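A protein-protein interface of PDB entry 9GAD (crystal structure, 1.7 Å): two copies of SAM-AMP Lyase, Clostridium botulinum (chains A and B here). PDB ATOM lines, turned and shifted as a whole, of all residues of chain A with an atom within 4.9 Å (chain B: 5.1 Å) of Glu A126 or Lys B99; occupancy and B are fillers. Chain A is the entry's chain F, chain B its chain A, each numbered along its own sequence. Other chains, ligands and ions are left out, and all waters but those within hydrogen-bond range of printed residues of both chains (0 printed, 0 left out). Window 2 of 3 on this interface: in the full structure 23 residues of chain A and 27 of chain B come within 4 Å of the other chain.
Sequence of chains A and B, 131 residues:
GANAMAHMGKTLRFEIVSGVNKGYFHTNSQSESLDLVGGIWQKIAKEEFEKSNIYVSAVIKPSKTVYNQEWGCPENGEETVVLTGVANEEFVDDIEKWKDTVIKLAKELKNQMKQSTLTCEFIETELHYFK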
ATOM      1  N   MET A   8       6.526  11.383 -18.425  1.00  0.00           N
ATOM      2  CA  MET A   8       5.637  12.020 -17.469  1.00  0.00           C
ATOM      3  C   MET A   8       5.201  13.387 -18.005  1.00  0.00           C
ATOM      4  O   MET A   8       6.038  14.173 -18.440  1.00  0.00           O
ATOM      5  CB  MET A   8       6.296  12.196 -16.092  1.00  0.00           C
ATOM      6  CG  MET A   8       5.540  13.113 -15.112  1.00  0.00           C
ATOM      7  SD  MET A   8       6.426  13.489 -13.577  1.00  0.00           S
ATOM      8  CE  MET A   8       7.740  14.572 -14.164  1.00  0.00           C
ATOM      9  N   GLY A   9       3.902  13.674 -17.971  1.00  0.00           N
ATOM     10  CA  GLY A   9       3.452  15.029 -18.284  1.00  0.00           C
ATOM     11  C   GLY A   9       2.071  15.342 -17.711  1.00  0.00           C
ATOM     12  O   GLY A   9       1.230  14.459 -17.486  1.00  0.00           O
ATOM     13  N   LYS A  10       1.828  16.647 -17.512  1.00  0.00           N
ATOM     14  CA  LYS A  10       0.536  17.128 -17.037  1.00  0.00           C
ATOM     15  C   LYS A  10      -0.463  17.177 -18.196  1.00  0.00           C
ATOM     16  O   LYS A  10      -0.085  17.586 -19.298  1.00  0.00           O
ATOM     17  CB  LYS A  10       0.821  18.466 -16.347  1.00  0.00           C
ATOM     18  CG  LYS A  10       1.124  18.329 -14.865  1.00  0.00           C
ATOM     19  CD  LYS A  10      -0.222  18.415 -14.149  1.00  0.00           C
ATOM     20  CE  LYS A  10      -0.309  18.127 -12.676  1.00  0.00           C
ATOM     21  NZ  LYS A  10      -1.665  17.613 -12.432  1.00  0.00           N
ATOM     22  N   GLU A 124      -7.817  17.280 -14.251  1.00  0.00           N
ATOM     23  CA  GLU A 124      -6.375  17.440 -14.443  1.00  0.00           C
ATOM     24  C   GLU A 124      -5.649  16.224 -13.856  1.00  0.00           C
ATOM     25  O   GLU A 124      -5.971  15.819 -12.740  1.00  0.00           O
ATOM     26  CB  GLU A 124      -5.898  18.716 -13.759  1.00  0.00           C
ATOM     27  CG  GLU A 124      -6.622  19.946 -14.301  1.00  0.00           C
ATOM     28  CD  GLU A 124      -5.913  21.267 -14.174  1.00  0.00           C
ATOM     29  OE1 GLU A 124      -4.816  21.364 -13.596  1.00  0.00           O
ATOM     30  OE2 GLU A 124      -6.540  22.177 -14.746  1.00  0.00           O
ATOM     31  N   THR A 125      -4.649  15.719 -14.597  1.00  0.00           N
ATOM     32  CA  THR A 125      -3.944  14.505 -14.202  1.00  0.00           C
ATOM     33  C   THR A 125      -2.483  14.592 -14.639  1.00  0.00           C
ATOM     34  O   THR A 125      -2.133  15.285 -15.599  1.00  0.00           O
ATOM     35  CB  THR A 125      -4.662  13.290 -14.787  1.00  0.00           C
ATOM     36  OG1 THR A 125      -4.098  12.100 -14.229  1.00  0.00           O
ATOM     37  CG2 THR A 125      -4.597  13.221 -16.303  1.00  0.00           C
ATOM     38  N   GLU A 126      -1.626  13.881 -13.897  1.00  0.00           N
ATOM     39  CA  GLU A 126      -0.213  13.717 -14.228  1.00  0.00           C
ATOM     40  C   GLU A 126      -0.019  12.264 -14.694  1.00  0.00           C
ATOM     41  O   GLU A 126      -0.082  11.369 -13.867  1.00  0.00           O
ATOM     42  CB  GLU A 126       0.666  14.038 -13.026  1.00  0.00           C
ATOM     43  CG  GLU A 126       2.166  13.908 -13.320  1.00  0.00           C
ATOM     44  CD  GLU A 126       3.018  14.121 -12.097  1.00  0.00           C
ATOM     45  OE1 GLU A 126       3.523  13.156 -11.464  1.00  0.00           O
ATOM     46  OE2 GLU A 126       3.207  15.316 -11.795  1.00  0.00           O
ATOM     47  N   LEU A 127       0.178  12.076 -15.998  1.00  0.00           N
ATOM     48  CA  LEU A 127       0.225  10.794 -16.662  1.00  0.00           C
ATOM     49  C   LEU A 127       1.677  10.334 -16.759  1.00  0.00           C
ATOM     50  O   LEU A 127       2.520  11.003 -17.386  1.00  0.00           O
ATOM     51  CB  LEU A 127      -0.389  10.849 -18.057  1.00  0.00           C
ATOM     52  CG  LEU A 127      -0.269   9.576 -18.891  1.00  0.00           C
ATOM     53  CD1 LEU A 127      -1.052   8.436 -18.208  1.00  0.00           C
ATOM     54  CD2 LEU A 127      -0.730   9.850 -20.357  1.00  0.00           C
ATOM     55  N   HIS A 128       1.944   9.141 -16.188  1.00  0.00           N
ATOM     56  CA  HIS A 128       3.201   8.432 -16.434  1.00  0.00           C
ATOM     57  C   HIS A 128       2.930   7.231 -17.339  1.00  0.00           C
ATOM     58  O   HIS A 128       2.034   6.413 -17.062  1.00  0.00           O
ATOM     59  CB  HIS A 128       3.765   7.961 -15.091  1.00  0.00           C
ATOM     60  CG  HIS A 128       4.093   9.057 -14.167  1.00  0.00           C
ATOM     61  ND1 HIS A 128       5.390   9.315 -13.758  1.00  0.00           N
ATOM     62  CD2 HIS A 128       3.337   9.957 -13.542  1.00  0.00           C
ATOM     63  CE1 HIS A 128       5.365  10.305 -12.865  1.00  0.00           C
ATOM     64  NE2 HIS A 128       4.110  10.717 -12.716  1.00  0.00           N
ATOM     65  N   LEU B  12      -2.601  13.035  -2.799  1.00  0.00           N
ATOM     66  CA  LEU B  12      -2.614  12.452  -4.144  1.00  0.00           C
ATOM     67  C   LEU B  12      -3.310  11.092  -4.112  1.00  0.00           C
ATOM     68  O   LEU B  12      -3.103  10.316  -3.191  1.00  0.00           O
ATOM     69  CB  LEU B  12      -1.211  12.266  -4.740  1.00  0.00           C
ATOM     70  CG  LEU B  12      -0.392  13.518  -5.071  1.00  0.00           C
ATOM     71  CD1 LEU B  12       1.014  13.032  -5.473  1.00  0.00           C
ATOM     72  CD2 LEU B  12      -1.056  14.394  -6.132  1.00  0.00           C
ATOM     73  N   ILE B  95       5.145  12.381   1.050  1.00  0.00           N
ATOM     74  CA  ILE B  95       4.392  12.189  -0.178  1.00  0.00           C
ATOM     75  C   ILE B  95       5.339  11.821  -1.318  1.00  0.00           C
ATOM     76  O   ILE B  95       4.972  11.039  -2.184  1.00  0.00           O
ATOM     77  CB  ILE B  95       3.538  13.426  -0.536  1.00  0.00           C
ATOM     78  CG1 ILE B  95       2.563  13.121  -1.682  1.00  0.00           C
ATOM     79  CG2 ILE B  95       4.403  14.643  -0.877  1.00  0.00           C
ATOM     80  CD1 ILE B  95       1.442  12.187  -1.278  1.00  0.00           C
ATOM     81  N   GLU B  96       6.551  12.403  -1.334  1.00  0.00           N
ATOM     82  CA  GLU B  96       7.500  12.141  -2.405  1.00  0.00           C
ATOM     83  C   GLU B  96       7.957  10.680  -2.366  1.00  0.00           C
ATOM     84  O   GLU B  96       8.038  10.047  -3.411  1.00  0.00           O
ATOM     85  CB  GLU B  96       8.672  13.128  -2.388  1.00  0.00           C
ATOM     86  N   LYS B  97       8.221  10.141  -1.167  1.00  0.00           N
ATOM     87  CA  LYS B  97       8.621   8.745  -1.007  1.00  0.00           C
ATOM     88  C   LYS B  97       7.487   7.801  -1.452  1.00  0.00           C
ATOM     89  O   LYS B  97       7.722   6.797  -2.119  1.00  0.00           O
ATOM     90  CB  LYS B  97       9.025   8.410   0.432  1.00  0.00           C
ATOM     91  CG  LYS B  97      10.400   8.894   0.875  1.00  0.00           C
ATOM     92  CD  LYS B  97      10.794   8.448   2.278  1.00  0.00           C
ATOM     93  CE  LYS B  97      12.138   8.987   2.686  1.00  0.00           C
ATOM     94  NZ  LYS B  97      12.408   8.745   4.107  1.00  0.00           N
ATOM     95  N   TRP B  98       6.248   8.145  -1.081  1.00  0.00           N
ATOM     96  CA  TRP B  98       5.072   7.389  -1.482  1.00  0.00           C
ATOM     97  C   TRP B  98       4.939   7.351  -3.005  1.00  0.00           C
ATOM     98  O   TRP B  98       4.730   6.290  -3.596  1.00  0.00           O
ATOM     99  CB  TRP B  98       3.819   7.986  -0.819  1.00  0.00           C
ATOM    100  CG  TRP B  98       2.529   7.296  -1.188  1.00  0.00           C
ATOM    101  CD1 TRP B  98       1.955   6.229  -0.572  1.00  0.00           C
ATOM    102  CD2 TRP B  98       1.614   7.696  -2.250  1.00  0.00           C
ATOM    103  NE1 TRP B  98       0.763   5.918  -1.183  1.00  0.00           N
ATOM    104  CE2 TRP B  98       0.529   6.801  -2.208  1.00  0.00           C
ATOM    105  CE3 TRP B  98       1.616   8.715  -3.198  1.00  0.00           C
ATOM    106  CZ2 TRP B  98      -0.557   6.906  -3.078  1.00  0.00           C
ATOM    107  CZ3 TRP B  98       0.556   8.810  -4.081  1.00  0.00           C
ATOM    108  CH2 TRP B  98      -0.518   7.920  -4.016  1.00  0.00           C
ATOM    109  N   LYS B  99       5.084   8.513  -3.649  1.00  0.00           N
ATOM    110  CA  LYS B  99       4.947   8.602  -5.093  1.00  0.00           C
ATOM    111  C   LYS B  99       5.992   7.725  -5.787  1.00  0.00           C
ATOM    112  O   LYS B  99       5.681   7.000  -6.733  1.00  0.00           O
ATOM    113  CB  LYS B  99       4.975  10.096  -5.423  1.00  0.00           C
ATOM    114  CG  LYS B  99       4.684  10.412  -6.856  1.00  0.00           C
ATOM    115  CD  LYS B  99       4.479  11.914  -7.086  1.00  0.00           C
ATOM    116  CE  LYS B  99       4.275  12.081  -8.537  1.00  0.00           C
ATOM    117  NZ  LYS B  99       4.476  13.442  -9.029  1.00  0.00           N
ATOM    118  N   ASP B 100       7.246   7.796  -5.305  1.00  0.00           N
ATOM    119  CA  ASP B 100       8.317   6.946  -5.815  1.00  0.00           C
ATOM    120  C   ASP B 100       7.963   5.462  -5.664  1.00  0.00           C
ATOM    121  O   ASP B 100       8.200   4.663  -6.582  1.00  0.00           O
ATOM    122  CB  ASP B 100       9.639   7.312  -5.154  1.00  0.00           C
ATOM    123  CG  ASP B 100      10.283   8.618  -5.625  1.00  0.00           C
ATOM    124  OD1 ASP B 100       9.881   9.156  -6.685  1.00  0.00           O
ATOM    125  OD2 ASP B 100      11.174   9.123  -4.905  1.00  0.00           O
ATOM    126  N   THR B 101       7.345   5.094  -4.530  1.00  0.00           N
ATOM    127  CA  THR B 101       6.938   3.714  -4.275  1.00  0.00           C
ATOM    128  C   THR B 101       5.826   3.252  -5.222  1.00  0.00           C
ATOM    129  O   THR B 101       5.860   2.134  -5.737  1.00  0.00           O
ATOM    130  CB  THR B 101       6.492   3.543  -2.827  1.00  0.00           C
ATOM    131  OG1 THR B 101       7.583   3.953  -2.019  1.00  0.00           O
ATOM    132  CG2 THR B 101       6.106   2.115  -2.491  1.00  0.00           C
ATOM    133  N   VAL B 102       4.843   4.131  -5.484  1.00  0.00           N
ATOM    134  CA  VAL B 102       3.783   3.791  -6.421  1.00  0.00           C
ATOM    135  C   VAL B 102       4.363   3.533  -7.814  1.00  0.00           C
ATOM    136  O   VAL B 102       3.958   2.593  -8.493  1.00  0.00           O
ATOM    137  CB  VAL B 102       2.670   4.866  -6.445  1.00  0.00           C
ATOM    138  CG1 VAL B 102       1.659   4.579  -7.563  1.00  0.00           C
ATOM    139  CG2 VAL B 102       1.971   4.983  -5.107  1.00  0.00           C
ATOM    140  N   ILE B 103       5.301   4.388  -8.282  1.00  0.00           N
ATOM    141  CA  ILE B 103       5.939   4.227  -9.583  1.00  0.00           C
ATOM    142  C   ILE B 103       6.677   2.881  -9.652  1.00  0.00           C
ATOM    143  O   ILE B 103       6.574   2.154 -10.657  1.00  0.00           O
ATOM    144  CB  ILE B 103       6.831   5.455  -9.890  1.00  0.00           C
ATOM    145  CG1 ILE B 103       5.935   6.692 -10.146  1.00  0.00           C
ATOM    146  CG2 ILE B 103       7.774   5.185 -11.069  1.00  0.00           C
ATOM    147  CD1 ILE B 103       6.683   8.011 -10.126  1.00  0.00           C
ATOM    148  N   CYS B 120       0.119   5.029 -15.359  1.00  0.00           N
ATOM    149  CA  CYS B 120      -0.107   5.390 -13.960  1.00  0.00           C
ATOM    150  C   CYS B 120      -0.326   6.908 -13.853  1.00  0.00           C
ATOM    151  O   CYS B 120       0.552   7.684 -14.214  1.00  0.00           O
ATOM    152  CB  CYS B 120       1.097   4.958 -13.124  1.00  0.00           C
ATOM    153  SG  CYS B 120       0.972   5.268 -11.353  1.00  0.00           S
ATOM    154  N   GLU B 121      -1.489   7.321 -13.346  1.00  0.00           N
ATOM    155  CA  GLU B 121      -1.848   8.726 -13.202  1.00  0.00           C
ATOM    156  C   GLU B 121      -1.864   9.132 -11.742  1.00  0.00           C
ATOM    157  O   GLU B 121      -2.242   8.312 -10.902  1.00  0.00           O
ATOM    158  CB  GLU B 121      -3.231   9.006 -13.776  1.00  0.00           C
ATOM    159  CG  GLU B 121      -3.317   8.896 -15.298  1.00  0.00           C
ATOM    160  CD  GLU B 121      -4.745   8.903 -15.786  1.00  0.00           C
ATOM    161  OE1 GLU B 121      -5.389   9.969 -15.615  1.00  0.00           O
ATOM    162  OE2 GLU B 121      -5.195   7.842 -16.270  1.00  0.00           O
ATOM    163  N   PHE B 122      -1.457  10.381 -11.467  1.00  0.00           N
ATOM    164  CA  PHE B 122      -1.614  11.008 -10.165  1.00  0.00           C
ATOM    165  C   PHE B 122      -2.592  12.185 -10.298  1.00  0.00           C
ATOM    166  O   PHE B 122      -2.405  13.026 -11.193  1.00  0.00           O
ATOM    167  CB  PHE B 122      -0.292  11.459  -9.560  1.00  0.00           C
ATOM    168  CG  PHE B 122       0.665  10.297  -9.295  1.00  0.00           C
ATOM    169  CD1 PHE B 122       0.573   9.583  -8.108  1.00  0.00           C
ATOM    170  CD2 PHE B 122       1.624   9.903 -10.241  1.00  0.00           C
ATOM    171  CE1 PHE B 122       1.429   8.509  -7.854  1.00  0.00           C
ATOM    172  CE2 PHE B 122       2.475   8.819  -9.978  1.00  0.00           C
ATOM    173  CZ  PHE B 122       2.397   8.151  -8.780  1.00  0.00           C
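Among the printed residues, merely in contact across the chains: Thr A125 with Phe B122, Glu A126 with Cys B120, Glu A126 with Glu B121, Leu A127 with Cys B120, Leu A127 with Glu B121, His A128 with Ile B103 and His A128 with Phe B122.
Of chain B, only Lys B99, Cys B120, Glu B121 and Phe B122 come within 4 Å of Glu A126. Lys B99 touches just one residue of chain A: Glu A126 (2.6 Å). Of the printed residues of chain B, Leu A127 touches Cys B120 (3.8 Å) and Glu B121 (3.7 Å). Of the printed residues of chain B, Thr A125 touches Glu B121 and Phe B122. Of the printed residues of chain A, Cys B120 touches Glu A126, Leu A127 and His A128. Printed residues of chain A within 4 Å of Glu B121: Thr A125, Glu A126 and Leu A127. Printed residues of chain A within 4 Å of Phe B122: Thr A125, Glu A126 and His A128. Val B102 touches none of the printed residues of chain A. Lys A10 touches none of the printed residues of chain B. The nearest printed residue of chain A that does not touch Glu B121 is His A128 (4.8 Å).
A ring nitrogen (NE2) of His A128 sits close to the side-chain sulfur of Met A8 (3.7 Å). The backbone carbonyl oxygen (O) of Gly A9 is in hydrogen-bond range of the backbone NH (N) of Leu A127, 3.0 Å away. The side-chain carboxylate (OE1) of Glu A126 is in hydrogen-bond range of a ring nitrogen (NE2) of His A128, 2.8 Å away.
Hydrophobic or aromatic side chains of chain B that line the printed part of chain A: Ile B103 and Phe B122. Hydrophobic or aromatic side chains of chain A within 4 Å of the printed part of chain B: Leu A127 and His A128. Along chain A the printed residues that touch a printed residue of chain B span positions 125 to 128. Among the printed residues, Asp or Glu carboxylates within 4 Å of a Lys or Arg side-chain nitrogen of the other chain: Glu A126 with Lys B99 (2.6 Å).
The side-chain amino group of Lys B99 lies within salt-bridge range of the side-chain carboxylate of Glu A126 (2.6 Å). N of His A128 is in hydrogen-bond range of O of Cys B120, at 2.8 Å. OG1 of Thr A125 is in hydrogen-bond range of OE1 of Glu B121. N of Phe B122 is in hydrogen-bond range of O of Glu A126.
No position is printed for both chains. Of the 11 pairs that touch across the chains among the printed residues, none has its exchanged pair printed and touching as well.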
